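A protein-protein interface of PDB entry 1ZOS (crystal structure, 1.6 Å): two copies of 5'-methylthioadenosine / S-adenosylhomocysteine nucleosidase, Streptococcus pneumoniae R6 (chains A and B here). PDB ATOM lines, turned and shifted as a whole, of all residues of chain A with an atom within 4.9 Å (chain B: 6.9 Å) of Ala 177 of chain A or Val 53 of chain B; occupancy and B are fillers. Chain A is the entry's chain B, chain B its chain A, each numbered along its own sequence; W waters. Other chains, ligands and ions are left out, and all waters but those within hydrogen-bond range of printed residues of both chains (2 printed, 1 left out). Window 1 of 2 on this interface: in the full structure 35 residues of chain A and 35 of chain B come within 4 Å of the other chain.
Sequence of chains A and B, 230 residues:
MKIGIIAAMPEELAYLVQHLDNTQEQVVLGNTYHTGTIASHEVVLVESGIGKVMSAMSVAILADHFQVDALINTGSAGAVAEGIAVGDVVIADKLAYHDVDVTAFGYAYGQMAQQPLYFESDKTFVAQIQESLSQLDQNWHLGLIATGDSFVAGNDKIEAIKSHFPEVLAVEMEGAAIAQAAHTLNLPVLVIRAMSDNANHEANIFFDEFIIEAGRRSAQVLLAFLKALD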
ATOM      1  N   LYS A  52     -25.355  24.886 -18.578  1.00  0.00           N
ATOM      2  CA  LYS A  52     -24.685  23.761 -17.934  1.00  0.00           C
ATOM      3  C   LYS A  52     -24.453  22.568 -18.857  1.00  0.00           C
ATOM      4  O   LYS A  52     -23.350  22.032 -18.925  1.00  0.00           O
ATOM      5  CB  LYS A  52     -25.493  23.289 -16.722  1.00  0.00           C
ATOM      6  CG  LYS A  52     -25.615  24.310 -15.610  1.00  0.00           C
ATOM      7  CD  LYS A  52     -26.295  23.686 -14.406  1.00  0.00           C
ATOM      8  CE  LYS A  52     -26.540  24.706 -13.319  1.00  0.00           C
ATOM      9  NZ  LYS A  52     -27.205  24.067 -12.142  1.00  0.00           N
ATOM     10  N   SER A  55     -21.916  23.361 -21.983  1.00  0.00           N
ATOM     11  CA  SER A  55     -20.539  23.490 -21.534  1.00  0.00           C
ATOM     12  C   SER A  55     -19.982  22.160 -21.022  1.00  0.00           C
ATOM     13  O   SER A  55     -18.809  21.844 -21.246  1.00  0.00           O
ATOM     14  CB  SER A  55     -20.421  24.584 -20.464  1.00  0.00           C
ATOM     15  OG  SER A  55     -21.247  24.332 -19.346  1.00  0.00           O
ATOM     16  N   ALA A  56     -20.823  21.375 -20.352  1.00  0.00           N
ATOM     17  CA  ALA A  56     -20.400  20.077 -19.830  1.00  0.00           C
ATOM     18  C   ALA A  56     -20.030  19.145 -20.987  1.00  0.00           C
ATOM     19  O   ALA A  56     -19.038  18.419 -20.923  1.00  0.00           O
ATOM     20  CB  ALA A  56     -21.517  19.464 -18.981  1.00  0.00           C
ATOM     21  N   TYR A  97     -22.743  26.526  -7.497  1.00  0.00           N
ATOM     22  CA  TYR A  97     -24.041  26.722  -8.131  1.00  0.00           C
ATOM     23  C   TYR A  97     -24.948  27.505  -7.196  1.00  0.00           C
ATOM     24  O   TYR A  97     -25.028  27.194  -6.008  1.00  0.00           O
ATOM     25  CB  TYR A  97     -24.720  25.382  -8.408  1.00  0.00           C
ATOM     26  CG  TYR A  97     -24.061  24.535  -9.461  1.00  0.00           C
ATOM     27  CD1 TYR A  97     -23.544  23.280  -9.147  1.00  0.00           C
ATOM     28  CD2 TYR A  97     -23.993  24.969 -10.783  1.00  0.00           C
ATOM     29  CE1 TYR A  97     -22.981  22.469 -10.130  1.00  0.00           C
ATOM     30  CE2 TYR A  97     -23.432  24.168 -11.774  1.00  0.00           C
ATOM     31  CZ  TYR A  97     -22.931  22.924 -11.443  1.00  0.00           C
ATOM     32  OH  TYR A  97     -22.384  22.130 -12.424  1.00  0.00           O
ATOM     33  N   THR A 147     -22.737  30.041 -10.370  1.00  0.00           N
ATOM     34  CA  THR A 147     -23.318  29.602 -11.635  1.00  0.00           C
ATOM     35  C   THR A 147     -24.745  29.080 -11.516  1.00  0.00           C
ATOM     36  O   THR A 147     -25.120  28.488 -10.508  1.00  0.00           O
ATOM     37  CB  THR A 147     -22.461  28.465 -12.228  1.00  0.00           C
ATOM     38  OG1 THR A 147     -21.103  28.896 -12.332  1.00  0.00           O
ATOM     39  CG2 THR A 147     -22.961  28.060 -13.596  1.00  0.00           C
ATOM     40  N   GLU A 174     -22.040  28.922 -16.941  1.00  0.00           N
ATOM     41  CA  GLU A 174     -21.205  27.770 -17.275  1.00  0.00           C
ATOM     42  C   GLU A 174     -20.033  27.490 -16.344  1.00  0.00           C
ATOM     43  O   GLU A 174     -19.516  26.371 -16.328  1.00  0.00           O
ATOM     44  CB  GLU A 174     -20.633  27.907 -18.691  1.00  0.00           C
ATOM     45  CG  GLU A 174     -21.670  28.056 -19.796  1.00  0.00           C
ATOM     46  CD  GLU A 174     -22.121  29.489 -20.005  1.00  0.00           C
ATOM     47  OE1 GLU A 174     -23.216  29.681 -20.581  1.00  0.00           O
ATOM     48  OE2 GLU A 174     -21.382  30.424 -19.616  1.00  0.00           O
ATOM     49  N   GLY A 175     -19.610  28.496 -15.587  1.00  0.00           N
ATOM     50  CA  GLY A 175     -18.456  28.340 -14.708  1.00  0.00           C
ATOM     51  C   GLY A 175     -18.370  27.087 -13.851  1.00  0.00           C
ATOM     52  O   GLY A 175     -17.446  26.271 -13.997  1.00  0.00           O
ATOM     53  N   ALA A 176     -19.325  26.937 -12.941  1.00  0.00           N
ATOM     54  CA  ALA A 176     -19.342  25.789 -12.047  1.00  0.00           C
ATOM     55  C   ALA A 176     -19.582  24.484 -12.795  1.00  0.00           C
ATOM     56  O   ALA A 176     -19.150  23.425 -12.344  1.00  0.00           O
ATOM     57  CB  ALA A 176     -20.400  25.980 -10.971  1.00  0.00           C
ATOM     58  N   ALA A 177     -20.275  24.556 -13.929  1.00  0.00           N
ATOM     59  CA  ALA A 177     -20.541  23.358 -14.721  1.00  0.00           C
ATOM     60  C   ALA A 177     -19.226  22.842 -15.295  1.00  0.00           C
ATOM     61  O   ALA A 177     -18.931  21.646 -15.239  1.00  0.00           O
ATOM     62  CB  ALA A 177     -21.522  23.676 -15.847  1.00  0.00           C
ATOM     63  N   ILE A 178     -18.435  23.755 -15.850  1.00  0.00           N
ATOM     64  CA  ILE A 178     -17.145  23.391 -16.408  1.00  0.00           C
ATOM     65  C   ILE A 178     -16.223  22.919 -15.282  1.00  0.00           C
ATOM     66  O   ILE A 178     -15.481  21.955 -15.450  1.00  0.00           O
ATOM     67  CB  ILE A 178     -16.522  24.587 -17.168  1.00  0.00           C
ATOM     68  CG1 ILE A 178     -17.347  24.857 -18.433  1.00  0.00           C
ATOM     69  CG2 ILE A 178     -15.062  24.287 -17.527  1.00  0.00           C
ATOM     70  CD1 ILE A 178     -17.032  26.170 -19.136  1.00  0.00           C
ATOM     71  N   ALA A 179     -16.283  23.592 -14.134  1.00  0.00           N
ATOM     72  CA  ALA A 179     -15.459  23.214 -12.985  1.00  0.00           C
ATOM     73  C   ALA A 179     -15.877  21.835 -12.463  1.00  0.00           C
ATOM     74  O   ALA A 179     -15.025  21.029 -12.072  1.00  0.00           O
ATOM     75  CB  ALA A 179     -15.585  24.264 -11.876  1.00  0.00           C
ATOM     76  N   GLN A 180     -17.182  21.564 -12.456  1.00  0.00           N
ATOM     77  CA  GLN A 180     -17.678  20.269 -11.993  1.00  0.00           C
ATOM     78  C   GLN A 180     -17.201  19.167 -12.926  1.00  0.00           C
ATOM     79  O   GLN A 180     -16.748  18.115 -12.480  1.00  0.00           O
ATOM     80  CB  GLN A 180     -19.207  20.235 -11.948  1.00  0.00           C
ATOM     81  CG  GLN A 180     -19.748  18.932 -11.342  1.00  0.00           C
ATOM     82  CD  GLN A 180     -21.253  18.769 -11.500  1.00  0.00           C
ATOM     83  OE1 GLN A 180     -21.988  19.747 -11.620  1.00  0.00           O
ATOM     84  NE2 GLN A 180     -21.717  17.522 -11.481  1.00  0.00           N
ATOM     85  N   ALA A 181     -17.312  19.411 -14.228  1.00  0.00           N
ATOM     86  CA  ALA A 181     -16.894  18.429 -15.219  1.00  0.00           C
ATOM     87  C   ALA A 181     -15.392  18.187 -15.107  1.00  0.00           C
ATOM     88  O   ALA A 181     -14.930  17.048 -15.179  1.00  0.00           O
ATOM     89  CB  ALA A 181     -17.252  18.916 -16.620  1.00  0.00           C
ATOM     90  N   SER B  48     -24.290   7.539 -15.113  1.00  0.00           N
ATOM     91  CA  SER B  48     -23.715   8.871 -15.297  1.00  0.00           C
ATOM     92  C   SER B  48     -23.360   9.658 -14.050  1.00  0.00           C
ATOM     93  O   SER B  48     -22.376  10.399 -14.031  1.00  0.00           O
ATOM     94  CB  SER B  48     -24.684   9.731 -16.110  1.00  0.00           C
ATOM     95  OG  SER B  48     -25.886   9.939 -15.376  1.00  0.00           O
ATOM     96  N   GLY B  49     -24.168   9.498 -13.011  1.00  0.00           N
ATOM     97  CA  GLY B  49     -23.991  10.291 -11.815  1.00  0.00           C
ATOM     98  C   GLY B  49     -25.197  11.224 -11.879  1.00  0.00           C
ATOM     99  O   GLY B  49     -25.824  11.353 -12.932  1.00  0.00           O
ATOM    100  N   ILE B  50     -25.503  11.898 -10.779  1.00  0.00           N
ATOM    101  CA  ILE B  50     -26.673  12.767 -10.689  1.00  0.00           C
ATOM    102  C   ILE B  50     -26.533  14.179 -11.248  1.00  0.00           C
ATOM    103  O   ILE B  50     -25.480  14.801 -11.133  1.00  0.00           O
ATOM    104  CB  ILE B  50     -27.114  12.873  -9.212  1.00  0.00           C
ATOM    105  CG1 ILE B  50     -27.547  11.492  -8.712  1.00  0.00           C
ATOM    106  CG2 ILE B  50     -28.228  13.904  -9.045  1.00  0.00           C
ATOM    107  CD1 ILE B  50     -27.536  11.369  -7.204  1.00  0.00           C
ATOM    108  N   GLY B  51     -27.602  14.674 -11.868  1.00  0.00           N
ATOM    109  CA  GLY B  51     -27.591  16.041 -12.359  1.00  0.00           C
ATOM    110  C   GLY B  51     -27.386  16.312 -13.833  1.00  0.00           C
ATOM    111  O   GLY B  51     -27.047  15.426 -14.602  1.00  0.00           O
ATOM    112  N   LYS B  52     -27.582  17.571 -14.207  1.00  0.00           N
ATOM    113  CA  LYS B  52     -27.443  18.000 -15.593  1.00  0.00           C
ATOM    114  C   LYS B  52     -26.045  17.785 -16.168  1.00  0.00           C
ATOM    115  O   LYS B  52     -25.890  17.242 -17.259  1.00  0.00           O
ATOM    116  CB  LYS B  52     -27.802  19.481 -15.719  1.00  0.00           C
ATOM    117  CG  LYS B  52     -29.252  19.815 -15.424  1.00  0.00           C
ATOM    118  CD  LYS B  52     -29.505  21.299 -15.655  1.00  0.00           C
ATOM    119  CE  LYS B  52     -30.910  21.702 -15.255  1.00  0.00           C
ATOM    120  NZ  LYS B  52     -31.141  23.150 -15.540  1.00  0.00           N
ATOM    121  N   VAL B  53     -25.026  18.213 -15.432  1.00  0.00           N
ATOM    122  CA  VAL B  53     -23.658  18.088 -15.919  1.00  0.00           C
ATOM    123  C   VAL B  53     -23.201  16.649 -16.099  1.00  0.00           C
ATOM    124  O   VAL B  53     -22.688  16.283 -17.161  1.00  0.00           O
ATOM    125  CB  VAL B  53     -22.675  18.842 -14.990  1.00  0.00           C
ATOM    126  CG1 VAL B  53     -21.234  18.476 -15.324  1.00  0.00           C
ATOM    127  CG2 VAL B  53     -22.892  20.337 -15.139  1.00  0.00           C
ATOM    128  N   MET B  54     -23.393  15.825 -15.076  1.00  0.00           N
ATOM    129  CA  MET B  54     -22.964  14.438 -15.174  1.00  0.00           C
ATOM    130  C   MET B  54     -23.667  13.699 -16.309  1.00  0.00           C
ATOM    131  O   MET B  54     -23.022  12.997 -17.086  1.00  0.00           O
ATOM    132  CB  MET B  54     -23.193  13.708 -13.847  1.00  0.00           C
ATOM    133  CG  MET B  54     -22.434  14.318 -12.667  1.00  0.00           C
ATOM    134  SD  MET B  54     -20.658  14.580 -12.971  1.00  0.00           S
ATOM    135  CE  MET B  54     -20.044  12.879 -12.977  1.00  0.00           C
ATOM    136  N   SER B  55     -24.982  13.862 -16.414  1.00  0.00           N
ATOM    137  CA  SER B  55     -25.712  13.172 -17.472  1.00  0.00           C
ATOM    138  C   SER B  55     -25.332  13.694 -18.861  1.00  0.00           C
ATOM    139  O   SER B  55     -25.226  12.924 -19.818  1.00  0.00           O
ATOM    140  CB  SER B  55     -27.225  13.272 -17.233  1.00  0.00           C
ATOM    141  OG  SER B  55     -27.676  14.608 -17.139  1.00  0.00           O
ATOM    142  N   ALA B  56     -25.117  15.000 -18.966  1.00  0.00           N
ATOM    143  CA  ALA B  56     -24.724  15.600 -20.234  1.00  0.00           C
ATOM    144  C   ALA B  56     -23.371  15.021 -20.664  1.00  0.00           C
ATOM    145  O   ALA B  56     -23.161  14.719 -21.839  1.00  0.00           O
ATOM    146  CB  ALA B  56     -24.639  17.120 -20.087  1.00  0.00           C
ATOM    147  N   MET B  57     -22.454  14.864 -19.711  1.00  0.00           N
ATOM    148  CA  MET B  57     -21.140  14.309 -20.024  1.00  0.00           C
ATOM    149  C   MET B  57     -21.264  12.887 -20.562  1.00  0.00           C
ATOM    150  O   MET B  57     -20.586  12.518 -21.519  1.00  0.00           O
ATOM    151  CB  MET B  57     -20.234  14.306 -18.783  1.00  0.00           C
ATOM    152  CG  MET B  57     -19.771  15.691 -18.349  1.00  0.00           C
ATOM    153  SD  MET B  57     -18.548  15.611 -17.021  1.00  0.00           S
ATOM    154  CE  MET B  57     -19.579  15.500 -15.649  1.00  0.00           C
ATOM    155  N   SER B  58     -22.131  12.088 -19.948  1.00  0.00           N
ATOM    156  CA  SER B  58     -22.304  10.711 -20.399  1.00  0.00           C
ATOM    157  C   SER B  58     -22.821  10.676 -21.833  1.00  0.00           C
ATOM    158  O   SER B  58     -22.396   9.836 -22.624  1.00  0.00           O
ATOM    159  CB  SER B  58     -23.260   9.953 -19.473  1.00  0.00           C
ATOM    160  OG  SER B  58     -24.572  10.470 -19.569  1.00  0.00           O
ATOM    161  N   ASP B 149     -31.952  20.990 -11.621  1.00  0.00           N
ATOM    162  CA  ASP B 149     -30.787  20.568 -10.850  1.00  0.00           C
ATOM    163  C   ASP B 149     -31.084  20.655  -9.355  1.00  0.00           C
ATOM    164  O   ASP B 149     -30.251  21.098  -8.565  1.00  0.00           O
ATOM    165  CB  ASP B 149     -29.568  21.429 -11.199  1.00  0.00           C
ATOM    166  CG  ASP B 149     -28.487  20.651 -11.939  1.00  0.00           C
ATOM    167  OD1 ASP B 149     -28.668  19.439 -12.200  1.00  0.00           O
ATOM    168  OD2 ASP B 149     -27.439  21.256 -12.255  1.00  0.00           O
ATOM    169  N   MET B 173     -33.852  14.977 -12.279  1.00  0.00           N
ATOM    170  CA  MET B 173     -32.671  15.817 -12.473  1.00  0.00           C
ATOM    171  C   MET B 173     -31.784  15.580 -13.692  1.00  0.00           C
ATOM    172  O   MET B 173     -30.716  16.183 -13.795  1.00  0.00           O
ATOM    173  CB  MET B 173     -31.814  15.743 -11.203  1.00  0.00           C
ATOM    174  CG  MET B 173     -32.536  16.236  -9.955  1.00  0.00           C
ATOM    175  SD  MET B 173     -31.664  15.886  -8.403  1.00  0.00           S
ATOM    176  CE  MET B 173     -30.332  17.074  -8.507  1.00  0.00           C
ATOM    177  N   ALA B 177     -31.895  17.218 -19.572  1.00  0.00           N
ATOM    178  CA  ALA B 177     -30.474  17.412 -19.841  1.00  0.00           C
ATOM    179  C   ALA B 177     -30.035  16.421 -20.915  1.00  0.00           C
ATOM    180  O   ALA B 177     -29.364  16.786 -21.882  1.00  0.00           O
ATOM    181  CB  ALA B 177     -29.660  17.203 -18.569  1.00  0.00           C
HETATM  182  O   HOH W   1     -25.261  19.659 -12.636  1.00  0.00           O
HETATM  183  O   HOH W   2     -30.049  24.355 -13.057  1.00  0.00           O
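Printed residues of chain B within 4 Å of Lys 52 of chain A: Asp 149 (2.8 Å).
Printed residues of chain B within 4 Å of Ala 56 of chain A: Val 53 and Met 57.
Of the printed residues of chain B, Tyr 97 of chain A touches Val 53.
Printed residues of chain B within 4 Å of Ala 177 of chain A: Val 53 (3.7 Å).
Printed residues of chain B within 4 Å of Gln 180 of chain A: Val 53 and Met 54.
Of chain A, only Ala 56, Tyr 97, Ala 177 and Gln 180 come within 4 Å of Val 53 of chain B.
Ser 55 of chain B touches none of the printed residues of chain A.
Printed residues of chain A within 4 Å of Met 57 of chain B: Ala 56 (3.8 Å) and Ala 181 (3.6 Å).
The nearest printed residue of chain A that does not touch Val 53 of chain B is Lys 52 of chain A (4.2 Å).
The nearest printed residue of chain A that does not touch Met 54 of chain B is Ala 56 of chain A (5.7 Å).
OH of Tyr 97 of chain A sits at hydrogen-bond distance from OE1 of Gln 180 of chain A, 2.5 Å away.
OH of Tyr 97 of chain A lies within hydrogen-bond range of O of Ala 176 of chain A.
O of Lys 52 of chain A is in hydrogen-bond range of OG of Ser 55 of chain A (3.1 Å).
N of Lys 52 of chain B sits at hydrogen-bond distance from OD1 of Asp 149 of chain B (2.9 Å).
The side-chain sulfur (SD) of Met 54 of chain B sits at hydrogen-bond distance from the side-chain amide nitrogen (NE2) of Gln 180 of chain A, at 3.5 Å.
The side-chain carboxylate (OD2) of Asp 149 of chain B lies within salt-bridge range of the side-chain amino group (NZ) of Lys 52 of chain A, at 2.8 Å.
Positions printed for both chains: 52, 55, 56 and 177.
Of the 8 pairs that touch across the chains among the printed residues, none has its exchanged pair printed and touching as well.
Ala 56 of chain A touches Val 53 of chain B.
Ala 56 of chain A touches Met 57 of chain B.
CG2 of Val 53 of chain B touches OH of Tyr 97 of chain A (3.3 Å).
CG2 of Val 53 of chain B touches CB of Ala 177 of chain A, 3.7 Å away.
CB of Val 53 of chain B touches OE1 of Gln 180 of chain A (3.6 Å).
Met 57 of chain B touches Ala 181 of chain A.
Water W1 lies within hydrogen-bond range of OD2 of Asp 149 of chain B (2.7 Å), N of Val 53 of chain B (3.2 Å), OE1 of Gln 180 of chain A (3.4 Å) and N of Lys 52 of chain B (3.5 Å).
Water W2 lies within hydrogen-bond range of NZ of Lys 52 of chain B (3.0 Å) and NZ of Lys 52 of chain A (3.0 Å).
Of the 13 printed residues of chain A, 6 touch a printed residue of chain B.
Of the 14 printed residues of chain B, 4 touch a printed residue of chain A.
Hydrophobic or aromatic side chains of chain B that line the printed part of chain A: Val 53, Met 54 and Met 57.
Among the printed residues, 8 pairs touch across the chains.
Among the printed residues, Asp or Glu carboxylates within 4 Å of a Lys or Arg side-chain nitrogen of the other chain: Lys 52 of chain A with Asp 149 of chain B (2.8 Å).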
